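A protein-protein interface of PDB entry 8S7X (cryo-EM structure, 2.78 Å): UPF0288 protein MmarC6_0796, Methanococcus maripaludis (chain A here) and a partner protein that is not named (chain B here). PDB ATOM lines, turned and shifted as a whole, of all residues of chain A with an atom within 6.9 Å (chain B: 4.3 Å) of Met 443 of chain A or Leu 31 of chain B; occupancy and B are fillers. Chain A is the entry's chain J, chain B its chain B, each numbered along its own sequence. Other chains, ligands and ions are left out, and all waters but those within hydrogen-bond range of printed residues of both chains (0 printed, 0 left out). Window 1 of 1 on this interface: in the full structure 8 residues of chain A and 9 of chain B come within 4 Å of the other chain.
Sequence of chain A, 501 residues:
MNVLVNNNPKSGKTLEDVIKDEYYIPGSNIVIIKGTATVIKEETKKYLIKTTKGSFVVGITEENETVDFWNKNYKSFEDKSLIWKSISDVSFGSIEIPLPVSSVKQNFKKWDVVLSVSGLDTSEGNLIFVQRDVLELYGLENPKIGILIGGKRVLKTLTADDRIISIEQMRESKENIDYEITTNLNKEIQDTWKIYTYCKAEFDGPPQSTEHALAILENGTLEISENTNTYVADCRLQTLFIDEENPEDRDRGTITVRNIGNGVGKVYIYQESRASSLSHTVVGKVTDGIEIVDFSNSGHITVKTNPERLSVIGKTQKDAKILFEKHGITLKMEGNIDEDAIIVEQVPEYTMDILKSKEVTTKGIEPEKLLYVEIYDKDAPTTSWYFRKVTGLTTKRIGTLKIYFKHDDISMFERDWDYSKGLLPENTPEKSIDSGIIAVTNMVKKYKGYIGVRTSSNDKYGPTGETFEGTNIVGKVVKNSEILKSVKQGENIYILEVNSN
O of Met 443 of chain A lies close to O of Leu 31 of chain B (3.3 Å).
O of Glu 29 of chain B sits at hydrogen-bond distance from N of Glu 145 of chain B (2.9 Å).
The side-chain amino group of Lys 30 of chain B sits close to the backbone carbonyl oxygen of Arg 32 of chain B.
N of Leu 31 of chain B lies within hydrogen-bond range of O of Asp 143 of chain B (2.9 Å).
The backbone NH of Arg 32 of chain B is in hydrogen-bond range of the backbone carbonyl oxygen of Asp 143 of chain B.
N of Met 443 of chain A sits at hydrogen-bond distance from O of Leu 423 of chain A.
The backbone NH (N) of Val 444 of chain A lies close to the side-chain amide oxygen (OD1) of Asn 442 of chain A (3.3 Å).
CB of Pro 425 of chain A touches OE1 of Glu 29 of chain B (3.7 Å).
CD2 of Leu 31 of chain B touches CD of Pro 425 of chain A, 3.7 Å away.
Lys 30 of chain B touches Val 444 of chain A (O to CG2, 2.8 Å).
Val 444 of chain A touches Leu 31 of chain B.
Val 444 of chain A touches Arg 32 of chain B (O to C, 3.3 Å).
Of the printed residues of chain B, Pro 425 of chain A touches Glu 29 (3.7 Å) and Leu 31 (3.7 Å).
Met 443 of chain A touches just one residue of chain B: Leu 31 (3.3 Å).
Printed residues of chain A within 4 Å of Glu 29 of chain B: Pro 425.
Of the printed residues of chain A, Lys 30 of chain B touches Val 444 (2.8 Å).
Leu 31 of chain B touches just these residues of chain A: Pro 425 (3.7 Å), Met 443 (3.3 Å) and Val 444 (3.6 Å).
Printed residues of chain A within 4 Å of Arg 32 of chain B: Val 444.
Among the printed residues, no Asp or Glu carboxylate lies within 4 Å of a Lys or Arg side-chain nitrogen of the other chain.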
ATOM      1  N   SER A 420      -7.275  38.029  -7.999  1.00  0.00           N
ATOM      2  CA  SER A 420      -7.398  36.577  -8.099  1.00  0.00           C
ATOM      3  C   SER A 420      -6.368  36.051  -9.096  1.00  0.00           C
ATOM      4  O   SER A 420      -6.681  35.655 -10.219  1.00  0.00           O
ATOM      5  CB  SER A 420      -8.813  36.195  -8.505  1.00  0.00           C
ATOM      6  OG  SER A 420      -9.228  36.931  -9.639  1.00  0.00           O
ATOM      7  N   LYS A 421      -5.109  36.057  -8.664  1.00  0.00           N
ATOM      8  CA  LYS A 421      -4.013  35.593  -9.497  1.00  0.00           C
ATOM      9  C   LYS A 421      -3.365  34.329  -8.948  1.00  0.00           C
ATOM     10  O   LYS A 421      -3.315  33.310  -9.639  1.00  0.00           O
ATOM     11  CB  LYS A 421      -2.969  36.705  -9.656  1.00  0.00           C
ATOM     12  CG  LYS A 421      -3.556  38.033 -10.090  1.00  0.00           C
ATOM     13  CD  LYS A 421      -4.348  37.890 -11.380  1.00  0.00           C
ATOM     14  CE  LYS A 421      -3.453  38.028 -12.597  1.00  0.00           C
ATOM     15  NZ  LYS A 421      -3.542  39.386 -13.191  1.00  0.00           N
ATOM     16  N   GLY A 422      -2.884  34.354  -7.715  1.00  0.00           N
ATOM     17  CA  GLY A 422      -2.209  33.191  -7.179  1.00  0.00           C
ATOM     18  C   GLY A 422      -3.138  32.272  -6.422  1.00  0.00           C
ATOM     19  O   GLY A 422      -2.750  31.686  -5.409  1.00  0.00           O
ATOM     20  N   LEU A 423      -4.371  32.128  -6.908  1.00  0.00           N
ATOM     21  CA  LEU A 423      -5.391  31.359  -6.198  1.00  0.00           C
ATOM     22  C   LEU A 423      -5.188  29.857  -6.406  1.00  0.00           C
ATOM     23  O   LEU A 423      -6.030  29.148  -6.950  1.00  0.00           O
ATOM     24  CB  LEU A 423      -6.781  31.796  -6.638  1.00  0.00           C
ATOM     25  CG  LEU A 423      -7.305  33.060  -5.959  1.00  0.00           C
ATOM     26  CD1 LEU A 423      -8.738  33.314  -6.364  1.00  0.00           C
ATOM     27  CD2 LEU A 423      -7.191  32.943  -4.458  1.00  0.00           C
ATOM     28  N   LEU A 424      -4.038  29.380  -5.950  1.00  0.00           N
ATOM     29  CA  LEU A 424      -3.786  27.955  -5.928  1.00  0.00           C
ATOM     30  C   LEU A 424      -4.736  27.281  -4.943  1.00  0.00           C
ATOM     31  O   LEU A 424      -5.158  27.895  -3.962  1.00  0.00           O
ATOM     32  CB  LEU A 424      -2.341  27.675  -5.519  1.00  0.00           C
ATOM     33  CG  LEU A 424      -1.235  28.041  -6.503  1.00  0.00           C
ATOM     34  CD1 LEU A 424       0.113  27.749  -5.887  1.00  0.00           C
ATOM     35  CD2 LEU A 424      -1.395  27.269  -7.792  1.00  0.00           C
ATOM     36  N   PRO A 425      -5.102  26.028  -5.188  1.00  0.00           N
ATOM     37  CA  PRO A 425      -5.916  25.302  -4.206  1.00  0.00           C
ATOM     38  C   PRO A 425      -5.249  25.269  -2.844  1.00  0.00           C
ATOM     39  O   PRO A 425      -4.181  24.672  -2.689  1.00  0.00           O
ATOM     40  CB  PRO A 425      -6.027  23.899  -4.814  1.00  0.00           C
ATOM     41  CG  PRO A 425      -5.826  24.105  -6.266  1.00  0.00           C
ATOM     42  CD  PRO A 425      -4.875  25.246  -6.413  1.00  0.00           C
ATOM     43  N   VAL A 440     -13.963  30.393  -1.730  1.00  0.00           N
ATOM     44  CA  VAL A 440     -13.580  31.014  -2.991  1.00  0.00           C
ATOM     45  C   VAL A 440     -13.128  29.911  -3.931  1.00  0.00           C
ATOM     46  O   VAL A 440     -12.326  29.053  -3.544  1.00  0.00           O
ATOM     47  CB  VAL A 440     -12.461  32.053  -2.797  1.00  0.00           C
ATOM     48  CG1 VAL A 440     -12.253  32.848  -4.062  1.00  0.00           C
ATOM     49  CG2 VAL A 440     -12.789  32.976  -1.643  1.00  0.00           C
ATOM     50  N   THR A 441     -13.642  29.921  -5.155  1.00  0.00           N
ATOM     51  CA  THR A 441     -13.209  28.951  -6.150  1.00  0.00           C
ATOM     52  C   THR A 441     -11.798  29.292  -6.609  1.00  0.00           C
ATOM     53  O   THR A 441     -11.507  30.446  -6.933  1.00  0.00           O
ATOM     54  CB  THR A 441     -14.160  28.931  -7.342  1.00  0.00           C
ATOM     55  OG1 THR A 441     -13.731  29.891  -8.309  1.00  0.00           O
ATOM     56  CG2 THR A 441     -15.551  29.291  -6.903  1.00  0.00           C
ATOM     57  N   ASN A 442     -10.926  28.292  -6.638  1.00  0.00           N
ATOM     58  CA  ASN A 442      -9.527  28.520  -6.968  1.00  0.00           C
ATOM     59  C   ASN A 442      -9.347  28.546  -8.484  1.00  0.00           C
ATOM     60  O   ASN A 442     -10.313  28.545  -9.251  1.00  0.00           O
ATOM     61  CB  ASN A 442      -8.647  27.468  -6.299  1.00  0.00           C
ATOM     62  CG  ASN A 442      -9.200  26.076  -6.436  1.00  0.00           C
ATOM     63  OD1 ASN A 442      -9.683  25.691  -7.493  1.00  0.00           O
ATOM     64  ND2 ASN A 442      -9.121  25.303  -5.364  1.00  0.00           N
ATOM     65  N   MET A 443      -8.092  28.557  -8.934  1.00  0.00           N
ATOM     66  CA  MET A 443      -7.792  28.673 -10.356  1.00  0.00           C
ATOM     67  C   MET A 443      -8.152  27.423 -11.141  1.00  0.00           C
ATOM     68  O   MET A 443      -8.090  27.452 -12.374  1.00  0.00           O
ATOM     69  CB  MET A 443      -6.312  28.985 -10.561  1.00  0.00           C
ATOM     70  CG  MET A 443      -5.372  28.003  -9.889  1.00  0.00           C
ATOM     71  SD  MET A 443      -3.739  27.985 -10.644  1.00  0.00           S
ATOM     72  CE  MET A 443      -3.096  29.555 -10.087  1.00  0.00           C
ATOM     73  N   VAL A 444      -8.508  26.329 -10.467  1.00  0.00           N
ATOM     74  CA  VAL A 444      -8.860  25.102 -11.174  1.00  0.00           C
ATOM     75  C   VAL A 444     -10.102  25.306 -12.024  1.00  0.00           C
ATOM     76  O   VAL A 444     -10.149  24.897 -13.190  1.00  0.00           O
ATOM     77  CB  VAL A 444      -9.061  23.955 -10.171  1.00  0.00           C
ATOM     78  CG1 VAL A 444      -9.403  22.689 -10.905  1.00  0.00           C
ATOM     79  CG2 VAL A 444      -7.821  23.771  -9.336  1.00  0.00           C
ATOM     80  N   LYS A 445     -11.123  25.940 -11.464  1.00  0.00           N
ATOM     81  CA  LYS A 445     -12.395  26.095 -12.144  1.00  0.00           C
ATOM     82  C   LYS A 445     -12.380  27.316 -13.058  1.00  0.00           C
ATOM     83  O   LYS A 445     -11.484  28.157 -13.007  1.00  0.00           O
ATOM     84  CB  LYS A 445     -13.525  26.197 -11.124  1.00  0.00           C
ATOM     85  CG  LYS A 445     -13.612  24.999 -10.208  1.00  0.00           C
ATOM     86  CD  LYS A 445     -13.742  23.715 -11.003  1.00  0.00           C
ATOM     87  CE  LYS A 445     -13.966  22.526 -10.090  1.00  0.00           C
ATOM     88  NZ  LYS A 445     -13.406  21.273 -10.653  1.00  0.00           N
ATOM     89  N   LYS A 446     -13.395  27.395 -13.916  1.00  0.00           N
ATOM     90  CA  LYS A 446     -13.484  28.510 -14.852  1.00  0.00           C
ATOM     91  C   LYS A 446     -13.862  29.803 -14.140  1.00  0.00           C
ATOM     92  O   LYS A 446     -13.416  30.887 -14.528  1.00  0.00           O
ATOM     93  CB  LYS A 446     -14.489  28.181 -15.954  1.00  0.00           C
ATOM     94  CG  LYS A 446     -14.764  29.312 -16.926  1.00  0.00           C
ATOM     95  CD  LYS A 446     -15.861  28.921 -17.894  1.00  0.00           C
ATOM     96  CE  LYS A 446     -15.282  28.468 -19.220  1.00  0.00           C
ATOM     97  NZ  LYS A 446     -15.906  27.201 -19.688  1.00  0.00           N
ATOM     98  N   LYS A 448     -12.989  31.351 -11.370  1.00  0.00           N
ATOM     99  CA  LYS A 448     -12.012  31.529 -10.309  1.00  0.00           C
ATOM    100  C   LYS A 448     -12.241  32.862  -9.613  1.00  0.00           C
ATOM    101  O   LYS A 448     -12.441  33.888 -10.269  1.00  0.00           O
ATOM    102  CB  LYS A 448     -10.598  31.455 -10.882  1.00  0.00           C
ATOM    103  CG  LYS A 448      -9.548  32.169 -10.057  1.00  0.00           C
ATOM    104  CD  LYS A 448      -8.308  32.460 -10.881  1.00  0.00           C
ATOM    105  CE  LYS A 448      -8.644  33.295 -12.091  1.00  0.00           C
ATOM    106  NZ  LYS A 448      -7.434  33.694 -12.856  1.00  0.00           N
ATOM    107  N   GLY A 449     -12.226  32.844  -8.285  1.00  0.00           N
ATOM    108  CA  GLY A 449     -12.308  34.046  -7.495  1.00  0.00           C
ATOM    109  C   GLY A 449     -13.695  34.402  -7.005  1.00  0.00           C
ATOM    110  O   GLY A 449     -13.819  35.253  -6.119  1.00  0.00           O
ATOM    111  N   GLY A 470     -12.158  22.284  -6.425  1.00  0.00           N
ATOM    112  CA  GLY A 470     -12.124  23.607  -7.013  1.00  0.00           C
ATOM    113  C   GLY A 470     -12.544  24.727  -6.084  1.00  0.00           C
ATOM    114  O   GLY A 470     -12.725  25.861  -6.527  1.00  0.00           O
ATOM    115  N   ASN A 472     -11.645  26.491  -2.164  1.00  0.00           N
ATOM    116  CA  ASN A 472     -10.837  26.562  -0.957  1.00  0.00           C
ATOM    117  C   ASN A 472     -11.566  27.387   0.089  1.00  0.00           C
ATOM    118  O   ASN A 472     -11.970  28.524  -0.180  1.00  0.00           O
ATOM    119  CB  ASN A 472      -9.444  27.136  -1.233  1.00  0.00           C
ATOM    120  CG  ASN A 472      -9.459  28.255  -2.237  1.00  0.00           C
ATOM    121  OD1 ASN A 472      -8.610  28.315  -3.123  1.00  0.00           O
ATOM    122  ND2 ASN A 472     -10.419  29.157  -2.105  1.00  0.00           N
ATOM    123  N   GLU B  29      -2.975  16.788  -8.323  1.00  0.00           N
ATOM    124  CA  GLU B  29      -3.813  17.958  -8.118  1.00  0.00           C
ATOM    125  C   GLU B  29      -4.077  18.651  -9.447  1.00  0.00           C
ATOM    126  O   GLU B  29      -3.145  18.952 -10.195  1.00  0.00           O
ATOM    127  CB  GLU B  29      -3.143  18.923  -7.145  1.00  0.00           C
ATOM    128  CG  GLU B  29      -3.647  20.343  -7.239  1.00  0.00           C
ATOM    129  CD  GLU B  29      -3.135  21.215  -6.116  1.00  0.00           C
ATOM    130  OE1 GLU B  29      -3.605  21.049  -4.973  1.00  0.00           O
ATOM    131  OE2 GLU B  29      -2.260  22.067  -6.374  1.00  0.00           O
ATOM    132  N   LYS B  30      -5.347  18.903  -9.744  1.00  0.00           N
ATOM    133  CA  LYS B  30      -5.711  19.571 -10.979  1.00  0.00           C
ATOM    134  C   LYS B  30      -5.727  21.077 -10.767  1.00  0.00           C
ATOM    135  O   LYS B  30      -6.172  21.567  -9.728  1.00  0.00           O
ATOM    136  CB  LYS B  30      -7.065  19.078 -11.492  1.00  0.00           C
ATOM    137  CG  LYS B  30      -8.264  19.544 -10.713  1.00  0.00           C
ATOM    138  CD  LYS B  30      -9.545  19.189 -11.445  1.00  0.00           C
ATOM    139  CE  LYS B  30      -9.481  19.614 -12.900  1.00  0.00           C
ATOM    140  NZ  LYS B  30     -10.809  20.010 -13.431  1.00  0.00           N
ATOM    141  N   LEU B  31      -5.211  21.804 -11.753  1.00  0.00           N
ATOM    142  CA  LEU B  31      -5.040  23.243 -11.650  1.00  0.00           C
ATOM    143  C   LEU B  31      -5.739  24.014 -12.758  1.00  0.00           C
ATOM    144  O   LEU B  31      -5.657  25.245 -12.777  1.00  0.00           O
ATOM    145  CB  LEU B  31      -3.548  23.600 -11.646  1.00  0.00           C
ATOM    146  CG  LEU B  31      -2.711  22.966 -10.538  1.00  0.00           C
ATOM    147  CD1 LEU B  31      -1.240  23.076 -10.856  1.00  0.00           C
ATOM    148  CD2 LEU B  31      -3.016  23.621  -9.213  1.00  0.00           C
ATOM    149  N   ARG B  32      -6.411  23.334 -13.679  1.00  0.00           N
ATOM    150  CA  ARG B  32      -7.150  24.009 -14.733  1.00  0.00           C
ATOM    151  C   ARG B  32      -8.232  23.070 -15.236  1.00  0.00           C
ATOM    152  O   ARG B  32      -8.314  21.910 -14.832  1.00  0.00           O
ATOM    153  CB  ARG B  32      -6.234  24.449 -15.877  1.00  0.00           C
ATOM    154  CG  ARG B  32      -5.510  23.315 -16.561  1.00  0.00           C
ATOM    155  CD  ARG B  32      -4.290  23.820 -17.296  1.00  0.00           C
ATOM    156  NE  ARG B  32      -3.309  24.378 -16.377  1.00  0.00           N
ATOM    157  CZ  ARG B  32      -2.410  23.665 -15.718  1.00  0.00           C
ATOM    158  NH1 ARG B  32      -2.329  22.356 -15.858  1.00  0.00           N
ATOM    159  NH2 ARG B  32      -1.572  24.285 -14.894  1.00  0.00           N
ATOM    160  N   ASP B 143      -4.773  18.731 -17.457  1.00  0.00           N
ATOM    161  CA  ASP B 143      -5.540  19.352 -16.388  1.00  0.00           C
ATOM    162  C   ASP B 143      -4.827  19.364 -15.045  1.00  0.00           C
ATOM    163  O   ASP B 143      -5.240  20.109 -14.155  1.00  0.00           O
ATOM    164  CB  ASP B 143      -6.890  18.648 -16.224  1.00  0.00           C
ATOM    165  CG  ASP B 143      -7.929  19.140 -17.207  1.00  0.00           C
ATOM    166  OD1 ASP B 143      -7.567  19.887 -18.139  1.00  0.00           O
ATOM    167  OD2 ASP B 143      -9.113  18.782 -17.047  1.00  0.00           O
ATOM    168  N   GLU B 145      -1.187  19.040 -12.335  1.00  0.00           N
ATOM    169  CA  GLU B 145       0.046  19.761 -12.061  1.00  0.00           C
ATOM    170  C   GLU B 145       1.195  19.333 -12.959  1.00  0.00           C
ATOM    171  O   GLU B 145       2.247  19.976 -12.928  1.00  0.00           O
ATOM    172  CB  GLU B 145       0.446  19.569 -10.602  1.00  0.00           C
ATOM    173  CG  GLU B 145       0.742  18.133 -10.247  1.00  0.00           C
ATOM    174  CD  GLU B 145       0.684  17.886  -8.762  1.00  0.00           C
ATOM    175  OE1 GLU B 145       0.488  18.858  -8.005  1.00  0.00           O
ATOM    176  OE2 GLU B 145       0.837  16.721  -8.346  1.00  0.00           O
ATOM    177  N   ILE B 209       1.613  28.981 -13.568  1.00  0.00           N
ATOM    178  CA  ILE B 209       1.712  28.623 -12.148  1.00  0.00           C
ATOM    179  C   ILE B 209       2.665  29.589 -11.456  1.00  0.00           C
ATOM    180  O   ILE B 209       3.726  29.908 -12.018  1.00  0.00           O
ATOM    181  CB  ILE B 209       2.188  27.177 -12.002  1.00  0.00           C
ATOM    182  CG1 ILE B 209       1.244  26.228 -12.735  1.00  0.00           C
ATOM    183  CG2 ILE B 209       2.277  26.784 -10.553  1.00  0.00           C
ATOM    184  CD1 ILE B 209      -0.186  26.342 -12.289  1.00  0.00           C
ATOM    185  N   PRO B 210       2.335  30.091 -10.266  1.00  0.00           N
ATOM    186  CA  PRO B 210       3.258  30.989  -9.566  1.00  0.00           C
ATOM    187  C   PRO B 210       4.580  30.299  -9.261  1.00  0.00           C
ATOM    188  O   PRO B 210       4.640  29.089  -9.047  1.00  0.00           O
ATOM    189  CB  PRO B 210       2.501  31.346  -8.284  1.00  0.00           C
ATOM    190  CG  PRO B 210       1.072  31.119  -8.617  1.00  0.00           C
ATOM    191  CD  PRO B 210       1.048  29.967  -9.564  1.00  0.00           C
